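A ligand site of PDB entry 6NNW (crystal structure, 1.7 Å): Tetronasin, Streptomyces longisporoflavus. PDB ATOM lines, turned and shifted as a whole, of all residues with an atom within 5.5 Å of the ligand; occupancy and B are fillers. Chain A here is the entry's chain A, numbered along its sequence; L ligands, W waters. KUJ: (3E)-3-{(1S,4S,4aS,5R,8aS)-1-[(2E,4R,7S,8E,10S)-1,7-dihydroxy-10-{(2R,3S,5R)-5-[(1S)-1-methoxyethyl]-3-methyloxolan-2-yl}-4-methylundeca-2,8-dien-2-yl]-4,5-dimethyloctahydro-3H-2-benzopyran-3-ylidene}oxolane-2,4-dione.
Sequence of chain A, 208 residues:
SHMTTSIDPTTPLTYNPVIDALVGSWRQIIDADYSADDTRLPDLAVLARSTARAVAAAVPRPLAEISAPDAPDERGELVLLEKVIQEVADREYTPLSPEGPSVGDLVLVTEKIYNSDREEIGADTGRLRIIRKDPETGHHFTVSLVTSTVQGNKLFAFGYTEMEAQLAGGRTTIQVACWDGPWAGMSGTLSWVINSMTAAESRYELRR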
ATOM      1  N   GLN A  86     -29.802  13.011 -27.431  1.00  0.00           N
ATOM      2  CA  GLN A  86     -29.820  12.401 -26.111  1.00  0.00           C
ATOM      3  C   GLN A  86     -30.250  13.461 -25.115  1.00  0.00           C
ATOM      4  O   GLN A  86     -29.739  14.585 -25.154  1.00  0.00           O
ATOM      5  CB  GLN A  86     -28.454  11.798 -25.732  1.00  0.00           C
ATOM      6  CG  GLN A  86     -27.862  11.021 -26.935  1.00  0.00           C
ATOM      7  CD  GLN A  86     -26.977   9.812 -26.610  1.00  0.00           C
ATOM      8  OE1 GLN A  86     -26.421   9.212 -27.534  1.00  0.00           O
ATOM      9  NE2 GLN A  86     -26.834   9.459 -25.331  1.00  0.00           N
ATOM     10  N   VAL A  88     -31.128  14.335 -21.004  1.00  0.00           N
ATOM     11  CA  VAL A  88     -31.008  13.929 -19.607  1.00  0.00           C
ATOM     12  C   VAL A  88     -32.381  13.634 -19.030  1.00  0.00           C
ATOM     13  O   VAL A  88     -33.327  14.432 -19.165  1.00  0.00           O
ATOM     14  CB  VAL A  88     -30.289  15.029 -18.815  1.00  0.00           C
ATOM     15  CG1 VAL A  88     -30.286  14.685 -17.302  1.00  0.00           C
ATOM     16  CG2 VAL A  88     -28.862  15.227 -19.340  1.00  0.00           C
ATOM     17  N   ARG A  91     -30.477  13.156 -12.841  1.00  0.00           N
ATOM     18  CA  ARG A  91     -29.102  13.495 -12.506  1.00  0.00           C
ATOM     19  C   ARG A  91     -28.963  13.535 -11.003  1.00  0.00           C
ATOM     20  O   ARG A  91     -29.795  14.138 -10.329  1.00  0.00           O
ATOM     21  CB  ARG A  91     -28.709  14.846 -13.112  1.00  0.00           C
ATOM     22  CG  ARG A  91     -27.224  15.116 -13.044  1.00  0.00           C
ATOM     23  CD  ARG A  91     -26.891  16.517 -13.540  1.00  0.00           C
ATOM     24  NE  ARG A  91     -27.215  17.500 -12.509  1.00  0.00           N
ATOM     25  CZ  ARG A  91     -26.338  18.349 -11.989  1.00  0.00           C
ATOM     26  NH1 ARG A  91     -26.722  19.208 -11.055  1.00  0.00           N
ATOM     27  NH2 ARG A  91     -25.082  18.347 -12.432  1.00  0.00           N
ATOM     28  N   TYR A  93     -26.055  14.582  -8.095  1.00  0.00           N
ATOM     29  CA  TYR A  93     -24.803  15.315  -7.907  1.00  0.00           C
ATOM     30  C   TYR A  93     -24.894  16.103  -6.623  1.00  0.00           C
ATOM     31  O   TYR A  93     -25.770  16.964  -6.496  1.00  0.00           O
ATOM     32  CB  TYR A  93     -24.531  16.242  -9.076  1.00  0.00           C
ATOM     33  CG  TYR A  93     -23.372  17.189  -8.911  1.00  0.00           C
ATOM     34  CD1 TYR A  93     -22.140  16.750  -8.421  1.00  0.00           C
ATOM     35  CD2 TYR A  93     -23.483  18.513  -9.302  1.00  0.00           C
ATOM     36  CE1 TYR A  93     -21.051  17.645  -8.299  1.00  0.00           C
ATOM     37  CE2 TYR A  93     -22.412  19.398  -9.199  1.00  0.00           C
ATOM     38  CZ  TYR A  93     -21.202  18.970  -8.706  1.00  0.00           C
ATOM     39  OH  TYR A  93     -20.177  19.885  -8.607  1.00  0.00           O
ATOM     40  N   PRO A 101     -17.724  23.256  -9.212  1.00  0.00           N
ATOM     41  CA  PRO A 101     -17.194  21.896  -9.405  1.00  0.00           C
ATOM     42  C   PRO A 101     -15.747  21.809  -8.941  1.00  0.00           C
ATOM     43  O   PRO A 101     -14.968  22.763  -9.077  1.00  0.00           O
ATOM     44  CB  PRO A 101     -17.301  21.691 -10.915  1.00  0.00           C
ATOM     45  CG  PRO A 101     -18.353  22.656 -11.364  1.00  0.00           C
ATOM     46  CD  PRO A 101     -18.198  23.854 -10.467  1.00  0.00           C
ATOM     47  N   ASP A 105     -15.375  15.432  -7.551  1.00  0.00           N
ATOM     48  CA  ASP A 105     -16.828  15.421  -7.687  1.00  0.00           C
ATOM     49  C   ASP A 105     -17.293  14.230  -8.509  1.00  0.00           C
ATOM     50  O   ASP A 105     -16.612  13.783  -9.441  1.00  0.00           O
ATOM     51  CB  ASP A 105     -17.315  16.712  -8.372  1.00  0.00           C
ATOM     52  CG  ASP A 105     -17.636  17.813  -7.394  1.00  0.00           C
ATOM     53  OD1 ASP A 105     -17.847  17.514  -6.198  1.00  0.00           O
ATOM     54  OD2 ASP A 105     -17.674  18.987  -7.836  1.00  0.00           O
ATOM     55  N   VAL A 107     -20.790  12.563 -10.553  1.00  0.00           N
ATOM     56  CA  VAL A 107     -22.118  12.817 -11.117  1.00  0.00           C
ATOM     57  C   VAL A 107     -22.636  11.511 -11.672  1.00  0.00           C
ATOM     58  O   VAL A 107     -21.901  10.814 -12.394  1.00  0.00           O
ATOM     59  CB  VAL A 107     -22.082  13.895 -12.220  1.00  0.00           C
ATOM     60  CG1 VAL A 107     -23.447  14.017 -12.908  1.00  0.00           C
ATOM     61  CG2 VAL A 107     -21.674  15.242 -11.627  1.00  0.00           C
ATOM     62  N   VAL A 109     -25.791  10.138 -14.101  1.00  0.00           N
ATOM     63  CA  VAL A 109     -26.783  10.702 -15.002  1.00  0.00           C
ATOM     64  C   VAL A 109     -27.396   9.574 -15.814  1.00  0.00           C
ATOM     65  O   VAL A 109     -26.732   8.571 -16.106  1.00  0.00           O
ATOM     66  CB  VAL A 109     -26.135  11.777 -15.905  1.00  0.00           C
ATOM     67  CG1 VAL A 109     -25.032  11.121 -16.797  1.00  0.00           C
ATOM     68  CG2 VAL A 109     -27.177  12.515 -16.737  1.00  0.00           C
ATOM     69  N   GLU A 111     -30.002   9.058 -19.425  1.00  0.00           N
ATOM     70  CA  GLU A 111     -30.515   9.782 -20.576  1.00  0.00           C
ATOM     71  C   GLU A 111     -31.403   8.862 -21.386  1.00  0.00           C
ATOM     72  O   GLU A 111     -31.256   7.641 -21.353  1.00  0.00           O
ATOM     73  CB  GLU A 111     -29.420  10.279 -21.521  1.00  0.00           C
ATOM     74  CG  GLU A 111     -28.352  11.161 -20.905  1.00  0.00           C
ATOM     75  CD  GLU A 111     -27.390  11.651 -21.970  1.00  0.00           C
ATOM     76  OE1 GLU A 111     -27.376  12.867 -22.248  1.00  0.00           O
ATOM     77  OE2 GLU A 111     -26.687  10.789 -22.551  1.00  0.00           O
ATOM     78  N   ASP A 124     -29.118   5.463 -21.717  1.00  0.00           N
ATOM     79  CA  ASP A 124     -27.796   5.225 -21.176  1.00  0.00           C
ATOM     80  C   ASP A 124     -27.710   5.766 -19.755  1.00  0.00           C
ATOM     81  O   ASP A 124     -28.544   6.546 -19.310  1.00  0.00           O
ATOM     82  CB  ASP A 124     -26.680   5.790 -22.062  1.00  0.00           C
ATOM     83  CG  ASP A 124     -26.762   7.271 -22.293  1.00  0.00           C
ATOM     84  OD1 ASP A 124     -27.500   7.976 -21.583  1.00  0.00           O
ATOM     85  OD2 ASP A 124     -26.028   7.745 -23.206  1.00  0.00           O
ATOM     86  N   GLY A 126     -24.570   7.185 -17.030  1.00  0.00           N
ATOM     87  CA  GLY A 126     -23.181   7.619 -16.948  1.00  0.00           C
ATOM     88  C   GLY A 126     -22.728   7.816 -15.514  1.00  0.00           C
ATOM     89  O   GLY A 126     -23.500   8.280 -14.670  1.00  0.00           O
ATOM     90  N   LEU A 128     -19.630   9.878 -13.826  1.00  0.00           N
ATOM     91  CA  LEU A 128     -18.674  10.885 -14.241  1.00  0.00           C
ATOM     92  C   LEU A 128     -17.882  11.367 -13.031  1.00  0.00           C
ATOM     93  O   LEU A 128     -18.472  11.675 -11.990  1.00  0.00           O
ATOM     94  CB  LEU A 128     -19.380  12.078 -14.902  1.00  0.00           C
ATOM     95  CG  LEU A 128     -20.593  11.761 -15.813  1.00  0.00           C
ATOM     96  CD1 LEU A 128     -21.308  13.026 -16.310  1.00  0.00           C
ATOM     97  CD2 LEU A 128     -20.186  10.884 -16.993  1.00  0.00           C
ATOM     98  N   ARG A 129     -16.567  11.448 -13.153  1.00  0.00           N
ATOM     99  CA  ARG A 129     -15.735  11.915 -12.034  1.00  0.00           C
ATOM    100  C   ARG A 129     -14.818  13.029 -12.497  1.00  0.00           C
ATOM    101  O   ARG A 129     -14.168  12.898 -13.538  1.00  0.00           O
ATOM    102  CB  ARG A 129     -14.898  10.735 -11.476  1.00  0.00           C
ATOM    103  CG  ARG A 129     -13.921  11.127 -10.349  1.00  0.00           C
ATOM    104  CD  ARG A 129     -14.614  11.137  -8.995  1.00  0.00           C
ATOM    105  NE  ARG A 129     -15.016   9.799  -8.570  1.00  0.00           N
ATOM    106  CZ  ARG A 129     -15.580   9.514  -7.397  1.00  0.00           C
ATOM    107  NH1 ARG A 129     -15.832  10.476  -6.523  1.00  0.00           N
ATOM    108  NH2 ARG A 129     -15.906   8.257  -7.103  1.00  0.00           N
ATOM    109  N   ILE A 130     -14.739  14.141 -11.753  1.00  0.00           N
ATOM    110  CA  ILE A 130     -13.747  15.161 -12.063  1.00  0.00           C
ATOM    111  C   ILE A 130     -12.406  14.687 -11.512  1.00  0.00           C
ATOM    112  O   ILE A 130     -12.267  14.451 -10.319  1.00  0.00           O
ATOM    113  CB  ILE A 130     -14.126  16.530 -11.482  1.00  0.00           C
ATOM    114  CG1 ILE A 130     -15.429  17.027 -12.088  1.00  0.00           C
ATOM    115  CG2 ILE A 130     -13.026  17.535 -11.761  1.00  0.00           C
ATOM    116  CD1 ILE A 130     -15.841  18.417 -11.590  1.00  0.00           C
ATOM    117  N   THR A 142     -12.447  15.239 -16.779  1.00  0.00           N
ATOM    118  CA  THR A 142     -13.332  14.252 -16.185  1.00  0.00           C
ATOM    119  C   THR A 142     -13.108  12.907 -16.841  1.00  0.00           C
ATOM    120  O   THR A 142     -12.742  12.821 -18.015  1.00  0.00           O
ATOM    121  CB  THR A 142     -14.797  14.613 -16.353  1.00  0.00           C
ATOM    122  OG1 THR A 142     -15.127  14.622 -17.748  1.00  0.00           O
ATOM    123  CG2 THR A 142     -15.062  15.982 -15.784  1.00  0.00           C
ATOM    124  N   SER A 144     -15.242   9.208 -17.511  1.00  0.00           N
ATOM    125  CA  SER A 144     -16.632   8.766 -17.527  1.00  0.00           C
ATOM    126  C   SER A 144     -16.665   7.284 -17.862  1.00  0.00           C
ATOM    127  O   SER A 144     -15.821   6.791 -18.613  1.00  0.00           O
ATOM    128  CB  SER A 144     -17.484   9.508 -18.563  1.00  0.00           C
ATOM    129  OG  SER A 144     -16.801   9.555 -19.805  1.00  0.00           O
ATOM    130  N   VAL A 146     -19.780   4.916 -19.248  1.00  0.00           N
ATOM    131  CA  VAL A 146     -21.151   4.979 -19.738  1.00  0.00           C
ATOM    132  C   VAL A 146     -21.573   3.577 -20.138  1.00  0.00           C
ATOM    133  O   VAL A 146     -20.789   2.844 -20.775  1.00  0.00           O
ATOM    134  CB  VAL A 146     -21.298   5.952 -20.918  1.00  0.00           C
ATOM    135  CG1 VAL A 146     -22.766   6.009 -21.389  1.00  0.00           C
ATOM    136  CG2 VAL A 146     -20.824   7.329 -20.522  1.00  0.00           C
ATOM    137  N   THR A 161     -12.253  13.607 -20.785  1.00  0.00           N
ATOM    138  CA  THR A 161     -12.661  14.788 -21.548  1.00  0.00           C
ATOM    139  C   THR A 161     -12.467  16.053 -20.720  1.00  0.00           C
ATOM    140  O   THR A 161     -12.343  16.001 -19.494  1.00  0.00           O
ATOM    141  CB  THR A 161     -14.141  14.721 -21.977  1.00  0.00           C
ATOM    142  OG1 THR A 161     -14.977  14.665 -20.815  1.00  0.00           O
ATOM    143  CG2 THR A 161     -14.406  13.507 -22.857  1.00  0.00           C
ATOM    144  N   MET A 163     -13.923  19.569 -19.306  1.00  0.00           N
ATOM    145  CA  MET A 163     -15.251  20.048 -18.905  1.00  0.00           C
ATOM    146  C   MET A 163     -15.560  21.385 -19.551  1.00  0.00           C
ATOM    147  O   MET A 163     -16.633  21.564 -20.135  1.00  0.00           O
ATOM    148  CB  MET A 163     -15.331  20.161 -17.383  1.00  0.00           C
ATOM    149  CG  MET A 163     -16.681  20.673 -16.867  1.00  0.00           C
ATOM    150  SD  MET A 163     -16.632  21.050 -15.085  1.00  0.00           S
ATOM    151  CE  MET A 163     -15.842  22.670 -15.138  1.00  0.00           C
ATOM    152  N   GLN A 166     -16.514  21.235 -23.272  1.00  0.00           N
ATOM    153  CA  GLN A 166     -17.847  20.703 -23.539  1.00  0.00           C
ATOM    154  C   GLN A 166     -18.903  21.774 -23.294  1.00  0.00           C
ATOM    155  O   GLN A 166     -19.815  21.965 -24.112  1.00  0.00           O
ATOM    156  CB  GLN A 166     -18.124  19.464 -22.677  1.00  0.00           C
ATOM    157  CG  GLN A 166     -19.570  19.012 -22.800  1.00  0.00           C
ATOM    158  CD  GLN A 166     -19.898  17.667 -22.154  1.00  0.00           C
ATOM    159  OE1 GLN A 166     -21.006  17.163 -22.302  1.00  0.00           O
ATOM    160  NE2 GLN A 166     -18.943  17.088 -21.445  1.00  0.00           N
ATOM    161  N   LEU A 167     -18.780  22.510 -22.188  1.00  0.00           N
ATOM    162  CA  LEU A 167     -19.777  23.521 -21.823  1.00  0.00           C
ATOM    163  C   LEU A 167     -19.860  24.624 -22.861  1.00  0.00           C
ATOM    164  O   LEU A 167     -20.915  25.241 -23.021  1.00  0.00           O
ATOM    165  CB  LEU A 167     -19.447  24.130 -20.454  1.00  0.00           C
ATOM    166  CG  LEU A 167     -19.684  23.206 -19.257  1.00  0.00           C
ATOM    167  CD1 LEU A 167     -19.162  23.832 -17.968  1.00  0.00           C
ATOM    168  CD2 LEU A 167     -21.163  22.903 -19.130  1.00  0.00           C
ATOM    169  N   THR A 172     -17.160  16.663 -28.075  1.00  0.00           N
ATOM    170  CA  THR A 172     -16.590  15.881 -26.987  1.00  0.00           C
ATOM    171  C   THR A 172     -16.689  14.422 -27.386  1.00  0.00           C
ATOM    172  O   THR A 172     -17.727  14.002 -27.905  1.00  0.00           O
ATOM    173  CB  THR A 172     -17.344  16.165 -25.694  1.00  0.00           C
ATOM    174  OG1 THR A 172     -17.300  17.577 -25.436  1.00  0.00           O
ATOM    175  CG2 THR A 172     -16.720  15.437 -24.530  1.00  0.00           C
ATOM    176  N   ILE A 174     -15.793  10.150 -26.612  1.00  0.00           N
ATOM    177  CA  ILE A 174     -15.397   9.044 -25.743  1.00  0.00           C
ATOM    178  C   ILE A 174     -15.303   7.767 -26.582  1.00  0.00           C
ATOM    179  O   ILE A 174     -15.746   7.710 -27.740  1.00  0.00           O
ATOM    180  CB  ILE A 174     -16.348   8.864 -24.549  1.00  0.00           C
ATOM    181  CG1 ILE A 174     -17.758   8.434 -24.980  1.00  0.00           C
ATOM    182  CG2 ILE A 174     -16.439  10.197 -23.742  1.00  0.00           C
ATOM    183  CD1 ILE A 174     -18.690   8.289 -23.820  1.00  0.00           C
ATOM    184  N   LEU A 190     -17.870   7.648 -29.653  1.00  0.00           N
ATOM    185  CA  LEU A 190     -19.169   8.278 -29.445  1.00  0.00           C
ATOM    186  C   LEU A 190     -18.877   9.734 -29.168  1.00  0.00           C
ATOM    187  O   LEU A 190     -18.200  10.059 -28.184  1.00  0.00           O
ATOM    188  CB  LEU A 190     -19.913   7.643 -28.290  1.00  0.00           C
ATOM    189  CG  LEU A 190     -21.158   8.238 -27.656  1.00  0.00           C
ATOM    190  CD1 LEU A 190     -22.139   8.641 -28.731  1.00  0.00           C
ATOM    191  CD2 LEU A 190     -21.743   7.202 -26.709  1.00  0.00           C
ATOM    192  N   TRP A 192     -20.295  13.966 -29.216  1.00  0.00           N
ATOM    193  CA  TRP A 192     -21.493  14.785 -29.124  1.00  0.00           C
ATOM    194  C   TRP A 192     -21.123  16.256 -29.057  1.00  0.00           C
ATOM    195  O   TRP A 192     -19.987  16.630 -28.715  1.00  0.00           O
ATOM    196  CB  TRP A 192     -22.351  14.392 -27.906  1.00  0.00           C
ATOM    197  CG  TRP A 192     -21.723  14.683 -26.575  1.00  0.00           C
ATOM    198  CD1 TRP A 192     -21.865  15.827 -25.840  1.00  0.00           C
ATOM    199  CD2 TRP A 192     -20.889  13.813 -25.814  1.00  0.00           C
ATOM    200  NE1 TRP A 192     -21.164  15.732 -24.676  1.00  0.00           N
ATOM    201  CE2 TRP A 192     -20.544  14.485 -24.633  1.00  0.00           C
ATOM    202  CE3 TRP A 192     -20.369  12.518 -26.031  1.00  0.00           C
ATOM    203  CZ2 TRP A 192     -19.736  13.924 -23.647  1.00  0.00           C
ATOM    204  CZ3 TRP A 192     -19.567  11.953 -25.038  1.00  0.00           C
ATOM    205  CH2 TRP A 192     -19.249  12.651 -23.875  1.00  0.00           C
ATOM    206  N   ILE A 194     -23.177  19.599 -27.198  1.00  0.00           N
ATOM    207  CA  ILE A 194     -24.346  19.884 -26.375  1.00  0.00           C
ATOM    208  C   ILE A 194     -25.196  20.963 -27.033  1.00  0.00           C
ATOM    209  O   ILE A 194     -24.675  21.876 -27.698  1.00  0.00           O
ATOM    210  CB  ILE A 194     -23.943  20.286 -24.937  1.00  0.00           C
ATOM    211  CG1 ILE A 194     -23.301  21.662 -24.916  1.00  0.00           C
ATOM    212  CG2 ILE A 194     -23.010  19.222 -24.290  1.00  0.00           C
ATOM    213  CD1 ILE A 194     -23.139  22.198 -23.511  1.00  0.00           C
ATOM    214  N   SER A 196     -27.720  22.233 -24.847  1.00  0.00           N
ATOM    215  CA  SER A 196     -28.076  22.890 -23.593  1.00  0.00           C
ATOM    216  C   SER A 196     -27.445  22.076 -22.463  1.00  0.00           C
ATOM    217  O   SER A 196     -26.676  21.147 -22.713  1.00  0.00           O
ATOM    218  CB  SER A 196     -29.592  22.969 -23.442  1.00  0.00           C
ATOM    219  OG  SER A 196     -30.110  21.657 -23.189  1.00  0.00           O
ATOM    220  N   MET A 197     -27.799  22.401 -21.217  1.00  0.00           N
ATOM    221  CA  MET A 197     -27.307  21.576 -20.130  1.00  0.00           C
ATOM    222  C   MET A 197     -28.034  20.241 -20.022  1.00  0.00           C
ATOM    223  O   MET A 197     -27.620  19.393 -19.218  1.00  0.00           O
ATOM    224  CB  MET A 197     -27.445  22.329 -18.806  1.00  0.00           C
ATOM    225  CG  MET A 197     -26.665  23.621 -18.816  1.00  0.00           C
ATOM    226  SD  MET A 197     -24.927  23.329 -18.452  1.00  0.00           S
ATOM    227  CE  MET A 197     -24.868  24.016 -16.794  1.00  0.00           C
ATOM    228  N   THR A 198     -29.071  20.006 -20.818  1.00  0.00           N
ATOM    229  CA  THR A 198     -29.821  18.751 -20.721  1.00  0.00           C
ATOM    230  C   THR A 198     -30.053  18.040 -22.036  1.00  0.00           C
ATOM    231  O   THR A 198     -30.819  17.060 -22.061  1.00  0.00           O
ATOM    232  CB  THR A 198     -31.175  18.987 -20.041  1.00  0.00           C
ATOM    233  OG1 THR A 198     -31.912  19.971 -20.784  1.00  0.00           O
ATOM    234  CG2 THR A 198     -30.969  19.452 -18.589  1.00  0.00           C
ATOM    235  N   ALA A 199     -29.450  18.481 -23.139  1.00  0.00           N
ATOM    236  CA  ALA A 199     -29.652  17.785 -24.407  1.00  0.00           C
ATOM    237  C   ALA A 199     -28.402  17.907 -25.254  1.00  0.00           C
ATOM    238  O   ALA A 199     -27.677  18.905 -25.179  1.00  0.00           O
ATOM    239  CB  ALA A 199     -30.874  18.319 -25.167  1.00  0.00           C
ATOM    240  N   ALA A 200     -28.122  16.871 -26.056  1.00  0.00           N
ATOM    241  CA  ALA A 200     -26.951  16.872 -26.912  1.00  0.00           C
ATOM    242  C   ALA A 200     -27.275  16.122 -28.195  1.00  0.00           C
ATOM    243  O   ALA A 200     -28.172  15.275 -28.210  1.00  0.00           O
ATOM    244  CB  ALA A 200     -25.719  16.252 -26.240  1.00  0.00           C
ATOM    245  N   SER A 202     -25.601  13.503 -30.838  1.00  0.00           N
ATOM    246  CA  SER A 202     -24.497  12.548 -30.736  1.00  0.00           C
ATOM    247  C   SER A 202     -24.315  11.791 -32.057  1.00  0.00           C
ATOM    248  O   SER A 202     -25.165  11.801 -32.952  1.00  0.00           O
ATOM    249  CB  SER A 202     -24.712  11.552 -29.594  1.00  0.00           C
ATOM    250  OG  SER A 202     -25.899  10.778 -29.800  1.00  0.00           O
HETATM  251  C01 KUJ L   1     -25.170  14.384 -20.162  1.00  0.00           C
HETATM  252  C02 KUJ L   1     -24.165  14.980 -21.156  1.00  0.00           C
HETATM  253  C03 KUJ L   1     -24.214  16.297 -21.560  1.00  0.00           C
HETATM  254  C04 KUJ L   1     -25.311  17.273 -21.098  1.00  0.00           C
HETATM  255  C05 KUJ L   1     -26.164  17.578 -22.290  1.00  0.00           C
HETATM  256  C06 KUJ L   1     -24.538  18.511 -20.628  1.00  0.00           C
HETATM  257  C07 KUJ L   1     -23.714  18.141 -19.316  1.00  0.00           C
HETATM  258  C08 KUJ L   1     -23.259  19.504 -18.732  1.00  0.00           C
HETATM  259  C09 KUJ L   1     -22.883  19.438 -17.239  1.00  0.00           C
HETATM  260  C10 KUJ L   1     -21.799  20.167 -16.774  1.00  0.00           C
HETATM  261  C11 KUJ L   1     -21.394  20.149 -15.300  1.00  0.00           C
HETATM  262  C12 KUJ L   1     -20.834  21.539 -15.039  1.00  0.00           C
HETATM  263  C13 KUJ L   1     -20.295  19.111 -15.000  1.00  0.00           C
HETATM  264  C14 KUJ L   1     -19.838  17.012 -14.289  1.00  0.00           C
HETATM  265  C15 KUJ L   1     -18.950  16.101 -15.011  1.00  0.00           C
HETATM  266  C16 KUJ L   1     -18.437  16.897 -17.239  1.00  0.00           C
HETATM  267  C17 KUJ L   1     -18.131  15.246 -14.001  1.00  0.00           C
HETATM  268  C18 KUJ L   1     -19.142  17.985 -13.341  1.00  0.00           C
HETATM  269  C19 KUJ L   1     -19.818  19.099 -13.452  1.00  0.00           C
HETATM  270  C20 KUJ L   1     -21.106  19.103 -12.502  1.00  0.00           C
HETATM  271  C21 KUJ L   1     -23.061  14.004 -21.655  1.00  0.00           C
HETATM  272  C22 KUJ L   1     -23.814  12.966 -22.519  1.00  0.00           C
HETATM  273  C23 KUJ L   1     -24.258  13.569 -23.874  1.00  0.00           C
HETATM  274  C24 KUJ L   1     -24.867  12.516 -24.819  1.00  0.00           C
HETATM  275  C25 KUJ L   1     -23.832  11.403 -25.035  1.00  0.00           C
HETATM  276  C26 KUJ L   1     -23.474  10.736 -23.701  1.00  0.00           C
HETATM  277  C27 KUJ L   1     -22.504   9.569 -23.972  1.00  0.00           C
HETATM  278  C28 KUJ L   1     -22.841  11.791 -22.779  1.00  0.00           C
HETATM  279  C29 KUJ L   1     -22.255  11.276 -21.443  1.00  0.00           C
HETATM  280  C30 KUJ L   1     -23.288  10.553 -20.562  1.00  0.00           C
HETATM  281  C31 KUJ L   1     -21.657  12.408 -20.598  1.00  0.00           C
HETATM  282  C32 KUJ L   1     -20.370  12.715 -20.350  1.00  0.00           C
HETATM  283  C33 KUJ L   1     -19.984  13.956 -19.867  1.00  0.00           C
HETATM  284  C34 KUJ L   1     -18.462  13.902 -19.731  1.00  0.00           C
HETATM  285  C35 KUJ L   1     -19.240  11.967 -20.508  1.00  0.00           C
HETATM  286  O01 KUJ L   1     -24.674  14.529 -18.852  1.00  0.00           O
HETATM  287  O02 KUJ L   1     -20.639  17.897 -15.239  1.00  0.00           O
HETATM  288  O03 KUJ L   1     -18.067  16.809 -15.891  1.00  0.00           O
HETATM  289  O04 KUJ L   1     -22.204  19.948 -19.502  1.00  0.00           O
HETATM  290  O05 KUJ L   1     -22.522  13.441 -20.497  1.00  0.00           O
HETATM  291  O06 KUJ L   1     -20.581  14.968 -19.560  1.00  0.00           O
HETATM  292  O07 KUJ L   1     -18.086  12.609 -20.155  1.00  0.00           O
HETATM  293  O08 KUJ L   1     -19.189  10.813 -20.912  1.00  0.00           O
HETATM  294  O   HOH W   1     -15.236  11.969 -19.716  1.00  0.00           O
HETATM  295  O   HOH W   2     -22.822  16.328 -15.926  1.00  0.00           O
HETATM  296  O   HOH W   3     -25.444  16.013 -16.469  1.00  0.00           O
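O08 of the ligand is in hydrogen-bond range of OG of Ser 144, 2.9 Å away.
NE2 of Gln 166 sits at hydrogen-bond distance from O06 of the ligand (3.3 Å).
N of Thr 142 sits at hydrogen-bond distance from O of Thr 161, 2.8 Å away.
The side-chain carboxylate of Glu 111 lies within hydrogen-bond range of the side-chain amide nitrogen of Gln 86.
The backbone NH of Trp 192 is in hydrogen-bond range of the backbone carbonyl oxygen of Thr 172, 2.9 Å away.
The backbone NH of Leu 128 sits at hydrogen-bond distance from the backbone carbonyl oxygen of Val 107 (2.8 Å).
OH of Tyr 93 lies within hydrogen-bond range of OD2 of Asp 105 (2.8 Å).
The side-chain amide nitrogen of Gln 86 lies within hydrogen-bond range of the side-chain carboxylate of Asp 124 (2.8 Å).
OG of Ser 202 lies within hydrogen-bond range of OE1 of Gln 86 (2.8 Å).
The backbone NH (N) of Val 88 is in hydrogen-bond range of the backbone carbonyl oxygen (O) of Thr 198, at 2.9 Å.
Gln 86 touches the ligand.
Val 88 touches the ligand.
CE2 of Tyr 93 touches C20 of the ligand (3.6 Å).
Val 107 touches the ligand.
CG2 of Val 109 touches O01 of the ligand, at 3.8 Å.
Glu 111 touches the ligand.
OD2 of Asp 124 touches C26 of the ligand, at 3.96 Å.
Leu 128 touches the ligand.
Ile 130 touches the ligand.
Thr 142 touches the ligand.
CG2 of Val 146 touches O08 of the ligand, 3.9 Å away.
OG1 of Thr 161 touches C34 of the ligand (3.7 Å).
Leu 167 touches the ligand.
CD1 of Ile 174 touches O08 of the ligand, 3.9 Å away.
CD2 of Leu 190 touches C27 of the ligand, 3.7 Å away.
CH2 of Trp 192 touches C35 of the ligand, at 3.4 Å.
Ser 196 touches the ligand.
Met 197 touches the ligand.
Thr 198 touches the ligand (C to C05, 3.9 Å).
Ala 199 touches the ligand.
Ala 200 touches the ligand.
Hydrophobic or aromatic side chains that line the ligand: Val 88, Tyr 93, Val 107, Val 109, Leu 128, Ile 130, Val 146, Leu 167, Ile 174, Leu 190, Trp 192 and Ala 200.
Of the 32 residues printed, 23 come within 4 Å of the ligand.
The nearest printed residue that does not touch the ligand is Ile 194 (4.03 Å).
Water W1 lies within hydrogen-bond range of OG of Ser 144 (2.9 Å), OG1 of Thr 161 (2.9 Å), O07 of the ligand (3.0 Å) and O of Thr 142 (3.1 Å).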
